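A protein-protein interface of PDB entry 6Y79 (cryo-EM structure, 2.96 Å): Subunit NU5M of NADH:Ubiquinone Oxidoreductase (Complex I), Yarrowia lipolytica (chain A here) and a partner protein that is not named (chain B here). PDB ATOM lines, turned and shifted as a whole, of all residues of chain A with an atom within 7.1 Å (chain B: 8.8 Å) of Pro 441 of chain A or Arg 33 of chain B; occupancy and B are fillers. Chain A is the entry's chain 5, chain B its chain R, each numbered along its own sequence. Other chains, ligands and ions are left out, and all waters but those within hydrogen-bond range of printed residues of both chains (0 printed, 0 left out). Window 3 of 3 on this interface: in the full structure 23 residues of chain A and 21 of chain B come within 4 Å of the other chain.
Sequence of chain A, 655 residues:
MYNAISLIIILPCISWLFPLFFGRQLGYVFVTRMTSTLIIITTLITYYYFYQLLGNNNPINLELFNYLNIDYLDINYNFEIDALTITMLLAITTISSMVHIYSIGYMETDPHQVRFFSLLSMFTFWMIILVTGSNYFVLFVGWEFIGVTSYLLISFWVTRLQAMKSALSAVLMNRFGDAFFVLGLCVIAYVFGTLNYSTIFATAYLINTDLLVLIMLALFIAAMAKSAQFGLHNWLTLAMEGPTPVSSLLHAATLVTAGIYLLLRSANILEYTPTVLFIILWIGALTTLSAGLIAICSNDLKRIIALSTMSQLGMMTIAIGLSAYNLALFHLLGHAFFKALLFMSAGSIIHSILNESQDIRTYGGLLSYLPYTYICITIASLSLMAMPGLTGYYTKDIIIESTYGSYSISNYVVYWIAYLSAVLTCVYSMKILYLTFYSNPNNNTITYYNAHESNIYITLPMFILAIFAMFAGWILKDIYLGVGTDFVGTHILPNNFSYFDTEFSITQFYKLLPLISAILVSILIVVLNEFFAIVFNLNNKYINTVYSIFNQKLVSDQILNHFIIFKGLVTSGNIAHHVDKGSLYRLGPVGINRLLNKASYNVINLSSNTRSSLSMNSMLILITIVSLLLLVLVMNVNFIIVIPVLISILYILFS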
ATOM      1  N   ARG A 361       4.425 -18.746   8.413  1.00  0.00           N
ATOM      2  CA  ARG A 361       2.987 -18.701   8.642  1.00  0.00           C
ATOM      3  C   ARG A 361       2.236 -19.710   7.785  1.00  0.00           C
ATOM      4  O   ARG A 361       1.068 -19.996   8.062  1.00  0.00           O
ATOM      5  CB  ARG A 361       2.470 -17.298   8.342  1.00  0.00           C
ATOM      6  CG  ARG A 361       2.924 -16.225   9.305  1.00  0.00           C
ATOM      7  CD  ARG A 361       2.265 -14.918   8.926  1.00  0.00           C
ATOM      8  NE  ARG A 361       2.591 -14.564   7.549  1.00  0.00           N
ATOM      9  CZ  ARG A 361       3.317 -13.510   7.205  1.00  0.00           C
ATOM     10  NH1 ARG A 361       3.759 -12.691   8.136  1.00  0.00           N
ATOM     11  NH2 ARG A 361       3.581 -13.260   5.934  1.00  0.00           N
ATOM     12  N   THR A 362       2.867 -20.232   6.737  1.00  0.00           N
ATOM     13  CA  THR A 362       2.237 -21.168   5.823  1.00  0.00           C
ATOM     14  C   THR A 362       2.784 -22.577   5.973  1.00  0.00           C
ATOM     15  O   THR A 362       2.465 -23.449   5.163  1.00  0.00           O
ATOM     16  CB  THR A 362       2.435 -20.697   4.387  1.00  0.00           C
ATOM     17  OG1 THR A 362       3.812 -20.883   4.036  1.00  0.00           O
ATOM     18  CG2 THR A 362       2.086 -19.246   4.259  1.00  0.00           C
ATOM     19  N   TYR A 363       3.613 -22.824   6.982  1.00  0.00           N
ATOM     20  CA  TYR A 363       4.220 -24.143   7.094  1.00  0.00           C
ATOM     21  C   TYR A 363       3.302 -25.097   7.834  1.00  0.00           C
ATOM     22  O   TYR A 363       2.936 -26.153   7.310  1.00  0.00           O
ATOM     23  CB  TYR A 363       5.566 -24.062   7.805  1.00  0.00           C
ATOM     24  CG  TYR A 363       6.694 -23.506   6.972  1.00  0.00           C
ATOM     25  CD1 TYR A 363       6.542 -23.256   5.612  1.00  0.00           C
ATOM     26  CD2 TYR A 363       7.922 -23.241   7.550  1.00  0.00           C
ATOM     27  CE1 TYR A 363       7.585 -22.748   4.863  1.00  0.00           C
ATOM     28  CE2 TYR A 363       8.964 -22.739   6.813  1.00  0.00           C
ATOM     29  CZ  TYR A 363       8.795 -22.493   5.475  1.00  0.00           C
ATOM     30  OH  TYR A 363       9.856 -21.990   4.763  1.00  0.00           O
ATOM     31  N   GLY A 364       2.919 -24.742   9.049  1.00  0.00           N
ATOM     32  CA  GLY A 364       2.151 -25.642   9.877  1.00  0.00           C
ATOM     33  C   GLY A 364       3.021 -26.741  10.435  1.00  0.00           C
ATOM     34  O   GLY A 364       4.226 -26.748  10.278  1.00  0.00           O
ATOM     35  N   GLY A 365       2.374 -27.693  11.100  1.00  0.00           N
ATOM     36  CA  GLY A 365       3.104 -28.765  11.748  1.00  0.00           C
ATOM     37  C   GLY A 365       3.628 -29.774  10.745  1.00  0.00           C
ATOM     38  O   GLY A 365       2.941 -30.162   9.803  1.00  0.00           O
ATOM     39  N   LEU A 366       4.887 -30.177  10.938  1.00  0.00           N
ATOM     40  CA  LEU A 366       5.533 -31.153  10.071  1.00  0.00           C
ATOM     41  C   LEU A 366       6.404 -32.117  10.862  1.00  0.00           C
ATOM     42  O   LEU A 366       7.341 -32.700  10.310  1.00  0.00           O
ATOM     43  CB  LEU A 366       6.396 -30.473   9.009  1.00  0.00           C
ATOM     44  CG  LEU A 366       5.751 -29.651   7.901  1.00  0.00           C
ATOM     45  CD1 LEU A 366       6.823 -28.914   7.132  1.00  0.00           C
ATOM     46  CD2 LEU A 366       4.962 -30.549   6.984  1.00  0.00           C
ATOM     47  N   TYR A 438       5.554 -28.034  15.334  1.00  0.00           N
ATOM     48  CA  TYR A 438       4.643 -28.325  16.435  1.00  0.00           C
ATOM     49  C   TYR A 438       3.256 -27.736  16.256  1.00  0.00           C
ATOM     50  O   TYR A 438       2.323 -28.161  16.943  1.00  0.00           O
ATOM     51  CB  TYR A 438       5.204 -27.783  17.748  1.00  0.00           C
ATOM     52  CG  TYR A 438       6.499 -28.387  18.205  1.00  0.00           C
ATOM     53  CD1 TYR A 438       6.883 -29.661  17.814  1.00  0.00           C
ATOM     54  CD2 TYR A 438       7.337 -27.674  19.047  1.00  0.00           C
ATOM     55  CE1 TYR A 438       8.067 -30.202  18.250  1.00  0.00           C
ATOM     56  CE2 TYR A 438       8.516 -28.202  19.485  1.00  0.00           C
ATOM     57  CZ  TYR A 438       8.876 -29.463  19.084  1.00  0.00           C
ATOM     58  OH  TYR A 438      10.060 -29.979  19.536  1.00  0.00           O
ATOM     59  N   SER A 439       3.109 -26.748  15.384  1.00  0.00           N
ATOM     60  CA  SER A 439       1.879 -25.984  15.295  1.00  0.00           C
ATOM     61  C   SER A 439       0.771 -26.808  14.648  1.00  0.00           C
ATOM     62  O   SER A 439       0.995 -27.877  14.079  1.00  0.00           O
ATOM     63  CB  SER A 439       2.118 -24.701  14.504  1.00  0.00           C
ATOM     64  OG  SER A 439       0.920 -23.971  14.338  1.00  0.00           O
ATOM     65  N   ASN A 440      -0.452 -26.313  14.782  1.00  0.00           N
ATOM     66  CA  ASN A 440      -1.538 -26.834  13.977  1.00  0.00           C
ATOM     67  C   ASN A 440      -1.305 -26.423  12.526  1.00  0.00           C
ATOM     68  O   ASN A 440      -0.772 -25.339  12.277  1.00  0.00           O
ATOM     69  CB  ASN A 440      -2.878 -26.305  14.483  1.00  0.00           C
ATOM     70  CG  ASN A 440      -3.261 -26.888  15.826  1.00  0.00           C
ATOM     71  OD1 ASN A 440      -3.128 -28.090  16.055  1.00  0.00           O
ATOM     72  ND2 ASN A 440      -3.739 -26.037  16.726  1.00  0.00           N
ATOM     73  N   PRO A 441      -1.657 -27.272  11.559  1.00  0.00           N
ATOM     74  CA  PRO A 441      -1.236 -27.032  10.177  1.00  0.00           C
ATOM     75  C   PRO A 441      -1.919 -25.834   9.542  1.00  0.00           C
ATOM     76  O   PRO A 441      -3.087 -25.538   9.800  1.00  0.00           O
ATOM     77  CB  PRO A 441      -1.622 -28.330   9.461  1.00  0.00           C
ATOM     78  CG  PRO A 441      -2.639 -28.933  10.291  1.00  0.00           C
ATOM     79  CD  PRO A 441      -2.336 -28.567  11.694  1.00  0.00           C
ATOM     80  N   ASN A 442      -1.154 -25.123   8.716  1.00  0.00           N
ATOM     81  CA  ASN A 442      -1.638 -23.922   8.059  1.00  0.00           C
ATOM     82  C   ASN A 442      -1.744 -24.060   6.553  1.00  0.00           C
ATOM     83  O   ASN A 442      -2.465 -23.277   5.929  1.00  0.00           O
ATOM     84  CB  ASN A 442      -0.726 -22.730   8.379  1.00  0.00           C
ATOM     85  CG  ASN A 442      -0.742 -22.358   9.840  1.00  0.00           C
ATOM     86  OD1 ASN A 442      -1.791 -22.298  10.464  1.00  0.00           O
ATOM     87  ND2 ASN A 442       0.432 -22.106  10.398  1.00  0.00           N
ATOM     88  N   ASN A 443      -1.050 -25.022   5.958  1.00  0.00           N
ATOM     89  CA  ASN A 443      -1.092 -25.215   4.522  1.00  0.00           C
ATOM     90  C   ASN A 443      -2.307 -26.053   4.137  1.00  0.00           C
ATOM     91  O   ASN A 443      -3.003 -26.608   4.987  1.00  0.00           O
ATOM     92  CB  ASN A 443       0.195 -25.878   4.043  1.00  0.00           C
ATOM     93  CG  ASN A 443       0.628 -25.390   2.681  1.00  0.00           C
ATOM     94  OD1 ASN A 443      -0.132 -24.738   1.971  1.00  0.00           O
ATOM     95  ND2 ASN A 443       1.864 -25.684   2.319  1.00  0.00           N
ATOM     96  N   ASN A 444      -2.566 -26.137   2.834  1.00  0.00           N
ATOM     97  CA  ASN A 444      -3.653 -26.983   2.367  1.00  0.00           C
ATOM     98  C   ASN A 444      -3.255 -28.455   2.467  1.00  0.00           C
ATOM     99  O   ASN A 444      -2.085 -28.797   2.647  1.00  0.00           O
ATOM    100  CB  ASN A 444      -4.062 -26.607   0.942  1.00  0.00           C
ATOM    101  CG  ASN A 444      -2.914 -26.662  -0.050  1.00  0.00           C
ATOM    102  OD1 ASN A 444      -1.769 -26.942   0.299  1.00  0.00           O
ATOM    103  ND2 ASN A 444      -3.225 -26.397  -1.310  1.00  0.00           N
ATOM    104  N   TYR A 448       0.438 -31.808   2.706  1.00  0.00           N
ATOM    105  CA  TYR A 448       0.610 -32.822   3.727  1.00  0.00           C
ATOM    106  C   TYR A 448       0.453 -34.230   3.167  1.00  0.00           C
ATOM    107  O   TYR A 448       0.964 -35.185   3.760  1.00  0.00           O
ATOM    108  CB  TYR A 448      -0.367 -32.538   4.862  1.00  0.00           C
ATOM    109  CG  TYR A 448      -0.069 -31.216   5.529  1.00  0.00           C
ATOM    110  CD1 TYR A 448       1.039 -31.070   6.346  1.00  0.00           C
ATOM    111  CD2 TYR A 448      -0.873 -30.108   5.320  1.00  0.00           C
ATOM    112  CE1 TYR A 448       1.332 -29.880   6.954  1.00  0.00           C
ATOM    113  CE2 TYR A 448      -0.584 -28.901   5.926  1.00  0.00           C
ATOM    114  CZ  TYR A 448       0.526 -28.799   6.738  1.00  0.00           C
ATOM    115  OH  TYR A 448       0.833 -27.613   7.353  1.00  0.00           O
ATOM    116  N   ALA B  26      -6.459  -9.958   7.313  1.00  0.00           N
ATOM    117  CA  ALA B  26      -6.483 -10.653   8.593  1.00  0.00           C
ATOM    118  C   ALA B  26      -5.748 -11.982   8.527  1.00  0.00           C
ATOM    119  O   ALA B  26      -5.352 -12.511   9.568  1.00  0.00           O
ATOM    120  CB  ALA B  26      -7.930 -10.875   9.036  1.00  0.00           C
ATOM    121  N   ARG B  27      -5.588 -12.541   7.320  1.00  0.00           N
ATOM    122  CA  ARG B  27      -4.945 -13.844   7.163  1.00  0.00           C
ATOM    123  C   ARG B  27      -3.487 -13.835   7.615  1.00  0.00           C
ATOM    124  O   ARG B  27      -3.030 -14.789   8.256  1.00  0.00           O
ATOM    125  CB  ARG B  27      -5.062 -14.298   5.708  1.00  0.00           C
ATOM    126  CG  ARG B  27      -4.242 -15.515   5.337  1.00  0.00           C
ATOM    127  CD  ARG B  27      -4.708 -16.748   6.077  1.00  0.00           C
ATOM    128  NE  ARG B  27      -3.796 -17.865   5.872  1.00  0.00           N
ATOM    129  CZ  ARG B  27      -2.734 -18.110   6.632  1.00  0.00           C
ATOM    130  NH1 ARG B  27      -2.452 -17.311   7.654  1.00  0.00           N
ATOM    131  NH2 ARG B  27      -1.957 -19.153   6.375  1.00  0.00           N
ATOM    132  N   ILE B  30      -2.623 -13.294  11.883  1.00  0.00           N
ATOM    133  CA  ILE B  30      -2.868 -14.329  12.879  1.00  0.00           C
ATOM    134  C   ILE B  30      -2.148 -15.606  12.475  1.00  0.00           C
ATOM    135  O   ILE B  30      -2.349 -16.128  11.372  1.00  0.00           O
ATOM    136  CB  ILE B  30      -4.370 -14.570  13.074  1.00  0.00           C
ATOM    137  CG1 ILE B  30      -5.022 -13.296  13.606  1.00  0.00           C
ATOM    138  CG2 ILE B  30      -4.584 -15.690  14.056  1.00  0.00           C
ATOM    139  CD1 ILE B  30      -6.481 -13.168  13.287  1.00  0.00           C
ATOM    140  N   SER B  31      -1.312 -16.107  13.383  1.00  0.00           N
ATOM    141  CA  SER B  31      -0.616 -17.371  13.194  1.00  0.00           C
ATOM    142  C   SER B  31      -1.542 -18.560  13.405  1.00  0.00           C
ATOM    143  O   SER B  31      -1.516 -19.510  12.615  1.00  0.00           O
ATOM    144  CB  SER B  31       0.562 -17.460  14.161  1.00  0.00           C
ATOM    145  OG  SER B  31       1.547 -16.488  13.868  1.00  0.00           O
ATOM    146  N   ASN B  32      -2.355 -18.528  14.459  1.00  0.00           N
ATOM    147  CA  ASN B  32      -3.190 -19.666  14.828  1.00  0.00           C
ATOM    148  C   ASN B  32      -4.325 -19.853  13.826  1.00  0.00           C
ATOM    149  O   ASN B  32      -4.727 -18.922  13.132  1.00  0.00           O
ATOM    150  CB  ASN B  32      -3.757 -19.460  16.235  1.00  0.00           C
ATOM    151  CG  ASN B  32      -4.336 -20.729  16.832  1.00  0.00           C
ATOM    152  OD1 ASN B  32      -4.251 -21.805  16.243  1.00  0.00           O
ATOM    153  ND2 ASN B  32      -4.939 -20.606  18.006  1.00  0.00           N
ATOM    154  N   ARG B  33      -4.839 -21.078  13.745  1.00  0.00           N
ATOM    155  CA  ARG B  33      -5.950 -21.325  12.835  1.00  0.00           C
ATOM    156  C   ARG B  33      -7.284 -20.914  13.448  1.00  0.00           C
ATOM    157  O   ARG B  33      -8.046 -20.168  12.821  1.00  0.00           O
ATOM    158  CB  ARG B  33      -5.984 -22.792  12.417  1.00  0.00           C
ATOM    159  CG  ARG B  33      -4.901 -23.145  11.430  1.00  0.00           C
ATOM    160  CD  ARG B  33      -5.065 -22.329  10.158  1.00  0.00           C
ATOM    161  NE  ARG B  33      -6.266 -22.682   9.414  1.00  0.00           N
ATOM    162  CZ  ARG B  33      -6.712 -22.007   8.360  1.00  0.00           C
ATOM    163  NH1 ARG B  33      -6.055 -20.941   7.930  1.00  0.00           N
ATOM    164  NH2 ARG B  33      -7.811 -22.399   7.733  1.00  0.00           N
ATOM    165  N   GLN B  34      -7.580 -21.355  14.676  1.00  0.00           N
ATOM    166  CA  GLN B  34      -8.906 -21.105  15.237  1.00  0.00           C
ATOM    167  C   GLN B  34      -9.023 -19.686  15.796  1.00  0.00           C
ATOM    168  O   GLN B  34     -10.133 -19.150  15.876  1.00  0.00           O
ATOM    169  CB  GLN B  34      -9.270 -22.148  16.306  1.00  0.00           C
ATOM    170  CG  GLN B  34      -8.450 -22.174  17.599  1.00  0.00           C
ATOM    171  CD  GLN B  34      -9.022 -21.258  18.664  1.00  0.00           C
ATOM    172  OE1 GLN B  34     -10.217 -20.976  18.675  1.00  0.00           O
ATOM    173  NE2 GLN B  34      -8.163 -20.781  19.562  1.00  0.00           N
ATOM    174  N   LEU B  35      -7.897 -19.058  16.200  1.00  0.00           N
ATOM    175  CA  LEU B  35      -7.955 -17.625  16.507  1.00  0.00           C
ATOM    176  C   LEU B  35      -8.291 -16.839  15.256  1.00  0.00           C
ATOM    177  O   LEU B  35      -9.100 -15.900  15.298  1.00  0.00           O
ATOM    178  CB  LEU B  35      -6.645 -17.120  17.098  1.00  0.00           C
ATOM    179  CG  LEU B  35      -6.616 -15.742  17.832  1.00  0.00           C
ATOM    180  CD1 LEU B  35      -5.535 -15.728  18.906  1.00  0.00           C
ATOM    181  CD2 LEU B  35      -6.515 -14.431  16.975  1.00  0.00           C
ATOM    182  N   PHE B  36      -7.704 -17.239  14.126  1.00  0.00           N
ATOM    183  CA  PHE B  36      -8.003 -16.580  12.868  1.00  0.00           C
ATOM    184  C   PHE B  36      -9.450 -16.788  12.467  1.00  0.00           C
ATOM    185  O   PHE B  36     -10.087 -15.871  11.953  1.00  0.00           O
ATOM    186  CB  PHE B  36      -7.095 -17.082  11.753  1.00  0.00           C
ATOM    187  CG  PHE B  36      -7.452 -16.511  10.428  1.00  0.00           C
ATOM    188  CD1 PHE B  36      -7.493 -15.140  10.262  1.00  0.00           C
ATOM    189  CD2 PHE B  36      -7.785 -17.325   9.364  1.00  0.00           C
ATOM    190  CE1 PHE B  36      -7.856 -14.594   9.064  1.00  0.00           C
ATOM    191  CE2 PHE B  36      -8.137 -16.782   8.151  1.00  0.00           C
ATOM    192  CZ  PHE B  36      -8.168 -15.415   8.000  1.00  0.00           C
ATOM    193  N   ARG B  37      -9.997 -17.966  12.709  1.00  0.00           N
ATOM    194  CA  ARG B  37     -11.342 -18.186  12.211  1.00  0.00           C
ATOM    195  C   ARG B  37     -12.411 -17.682  13.158  1.00  0.00           C
ATOM    196  O   ARG B  37     -13.483 -17.284  12.689  1.00  0.00           O
ATOM    197  CB  ARG B  37     -11.519 -19.655  11.876  1.00  0.00           C
ATOM    198  CG  ARG B  37     -10.547 -20.018  10.796  1.00  0.00           C
ATOM    199  CD  ARG B  37     -10.860 -19.284   9.523  1.00  0.00           C
ATOM    200  NE  ARG B  37     -12.173 -19.665   9.036  1.00  0.00           N
ATOM    201  CZ  ARG B  37     -12.825 -19.029   8.074  1.00  0.00           C
ATOM    202  NH1 ARG B  37     -12.290 -17.971   7.484  1.00  0.00           N
ATOM    203  NH2 ARG B  37     -14.019 -19.451   7.709  1.00  0.00           N
ATOM    204  N   GLN B  38     -12.128 -17.639  14.465  1.00  0.00           N
ATOM    205  CA  GLN B  38     -12.915 -16.821  15.384  1.00  0.00           C
ATOM    206  C   GLN B  38     -12.948 -15.366  14.928  1.00  0.00           C
ATOM    207  O   GLN B  38     -14.017 -14.748  14.860  1.00  0.00           O
ATOM    208  CB  GLN B  38     -12.339 -16.925  16.798  1.00  0.00           C
ATOM    209  CG  GLN B  38     -12.706 -18.191  17.562  1.00  0.00           C
ATOM    210  CD  GLN B  38     -11.942 -18.312  18.871  1.00  0.00           C
ATOM    211  OE1 GLN B  38     -11.241 -17.388  19.278  1.00  0.00           O
ATOM    212  NE2 GLN B  38     -12.058 -19.462  19.525  1.00  0.00           N
ATOM    213  N   LYS B  39     -11.785 -14.821  14.557  1.00  0.00           N
ATOM    214  CA  LYS B  39     -11.705 -13.438  14.095  1.00  0.00           C
ATOM    215  C   LYS B  39     -12.408 -13.238  12.751  1.00  0.00           C
ATOM    216  O   LYS B  39     -13.009 -12.183  12.497  1.00  0.00           O
ATOM    217  CB  LYS B  39     -10.234 -13.039  14.003  1.00  0.00           C
ATOM    218  CG  LYS B  39      -9.984 -11.630  13.557  1.00  0.00           C
ATOM    219  CD  LYS B  39     -10.442 -10.661  14.611  1.00  0.00           C
ATOM    220  CE  LYS B  39     -10.175  -9.235  14.185  1.00  0.00           C
ATOM    221  NZ  LYS B  39     -10.639  -8.271  15.213  1.00  0.00           N
ATOM    222  N   ALA B  40     -12.355 -14.247  11.883  1.00  0.00           N
ATOM    223  CA  ALA B  40     -12.985 -14.145  10.574  1.00  0.00           C
ATOM    224  C   ALA B  40     -14.498 -14.186  10.686  1.00  0.00           C
ATOM    225  O   ALA B  40     -15.185 -13.416  10.008  1.00  0.00           O
ATOM    226  CB  ALA B  40     -12.489 -15.263   9.661  1.00  0.00           C
ATOM    227  N   VAL B  41     -15.031 -15.040  11.565  1.00  0.00           N
ATOM    228  CA  VAL B  41     -16.466 -15.023  11.833  1.00  0.00           C
ATOM    229  C   VAL B  41     -16.857 -13.731  12.548  1.00  0.00           C
ATOM    230  O   VAL B  41     -17.959 -13.209  12.339  1.00  0.00           O
ATOM    231  CB  VAL B  41     -16.863 -16.293  12.615  1.00  0.00           C
ATOM    232  CG1 VAL B  41     -18.326 -16.296  12.996  1.00  0.00           C
ATOM    233  CG2 VAL B  41     -16.595 -17.503  11.765  1.00  0.00           C
ATOM    234  N   ILE B  79       1.273 -12.601   2.620  1.00  0.00           N
ATOM    235  CA  ILE B  79       1.510 -13.991   2.249  1.00  0.00           C
ATOM    236  C   ILE B  79       1.232 -14.102   0.757  1.00  0.00           C
ATOM    237  O   ILE B  79       0.139 -13.760   0.314  1.00  0.00           O
ATOM    238  CB  ILE B  79       0.627 -14.950   3.052  1.00  0.00           C
ATOM    239  CG1 ILE B  79       1.067 -14.979   4.509  1.00  0.00           C
ATOM    240  CG2 ILE B  79       0.695 -16.339   2.472  1.00  0.00           C
ATOM    241  CD1 ILE B  79       0.164 -15.784   5.393  1.00  0.00           C
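The backbone carbonyl oxygen of Arg 361 of chain A lies within hydrogen-bond range of the side-chain amide nitrogen of Asn 442 of chain A. The backbone NH (N) of Asn 442 of chain A sits at hydrogen-bond distance from the side-chain hydroxyl (OH) of Tyr 448 of chain A.
Among the printed residues, pairs that only touch across the chains: Asn 442 of chain A with Arg 33 of chain B, Arg 361 of chain A with Ile 79 of chain B, Pro 441 of chain A with Arg 33 of chain B, Asn 442 of chain A with Ser 31 of chain B, Arg 361 of chain A with Arg 27 of chain B and Thr 362 of chain A with Ile 79 of chain B.
Pro 441 of chain A touches one residue of chain B. Arg 33 of chain B touches two residues of chain A. Of the printed residues of chain B, Thr 362 of chain A touches Ile 79 (3.7 Å). Of the printed residues of chain A, Arg 27 of chain B touches Arg 361 (3.6 Å). Of the printed residues of chain A, Ile 79 of chain B touches Arg 361 (3.4 Å) and Thr 362 (3.7 Å). Printed residues of chain A within 4 Å of Ser 31 of chain B: Asn 442. Printed residues of chain B within 4 Å of Arg 361 of chain A: Arg 27 and Ile 79. Arg 37 of chain B touches none of the printed residues of chain A. Ala 40 of chain B touches none of the printed residues of chain A. The nearest residue of chain A that does not touch Arg 33 of chain B is Asn 440 of chain A (4.8 Å).
Hydrophobic or aromatic side chains of chain B that line the printed part of chain A: Ile 79. Of the 14 printed residues of chain A, 4 touch a printed residue of chain B. Printed residues of chain A that touch a printed residue of chain B: Arg 361, Thr 362, Pro 441 and Asn 442. Among the printed residues, 6 pairs touch across the chains. Among the printed residues, no Asp or Glu carboxylate lies within 4 Å of a Lys or Arg side-chain nitrogen of the other chain.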
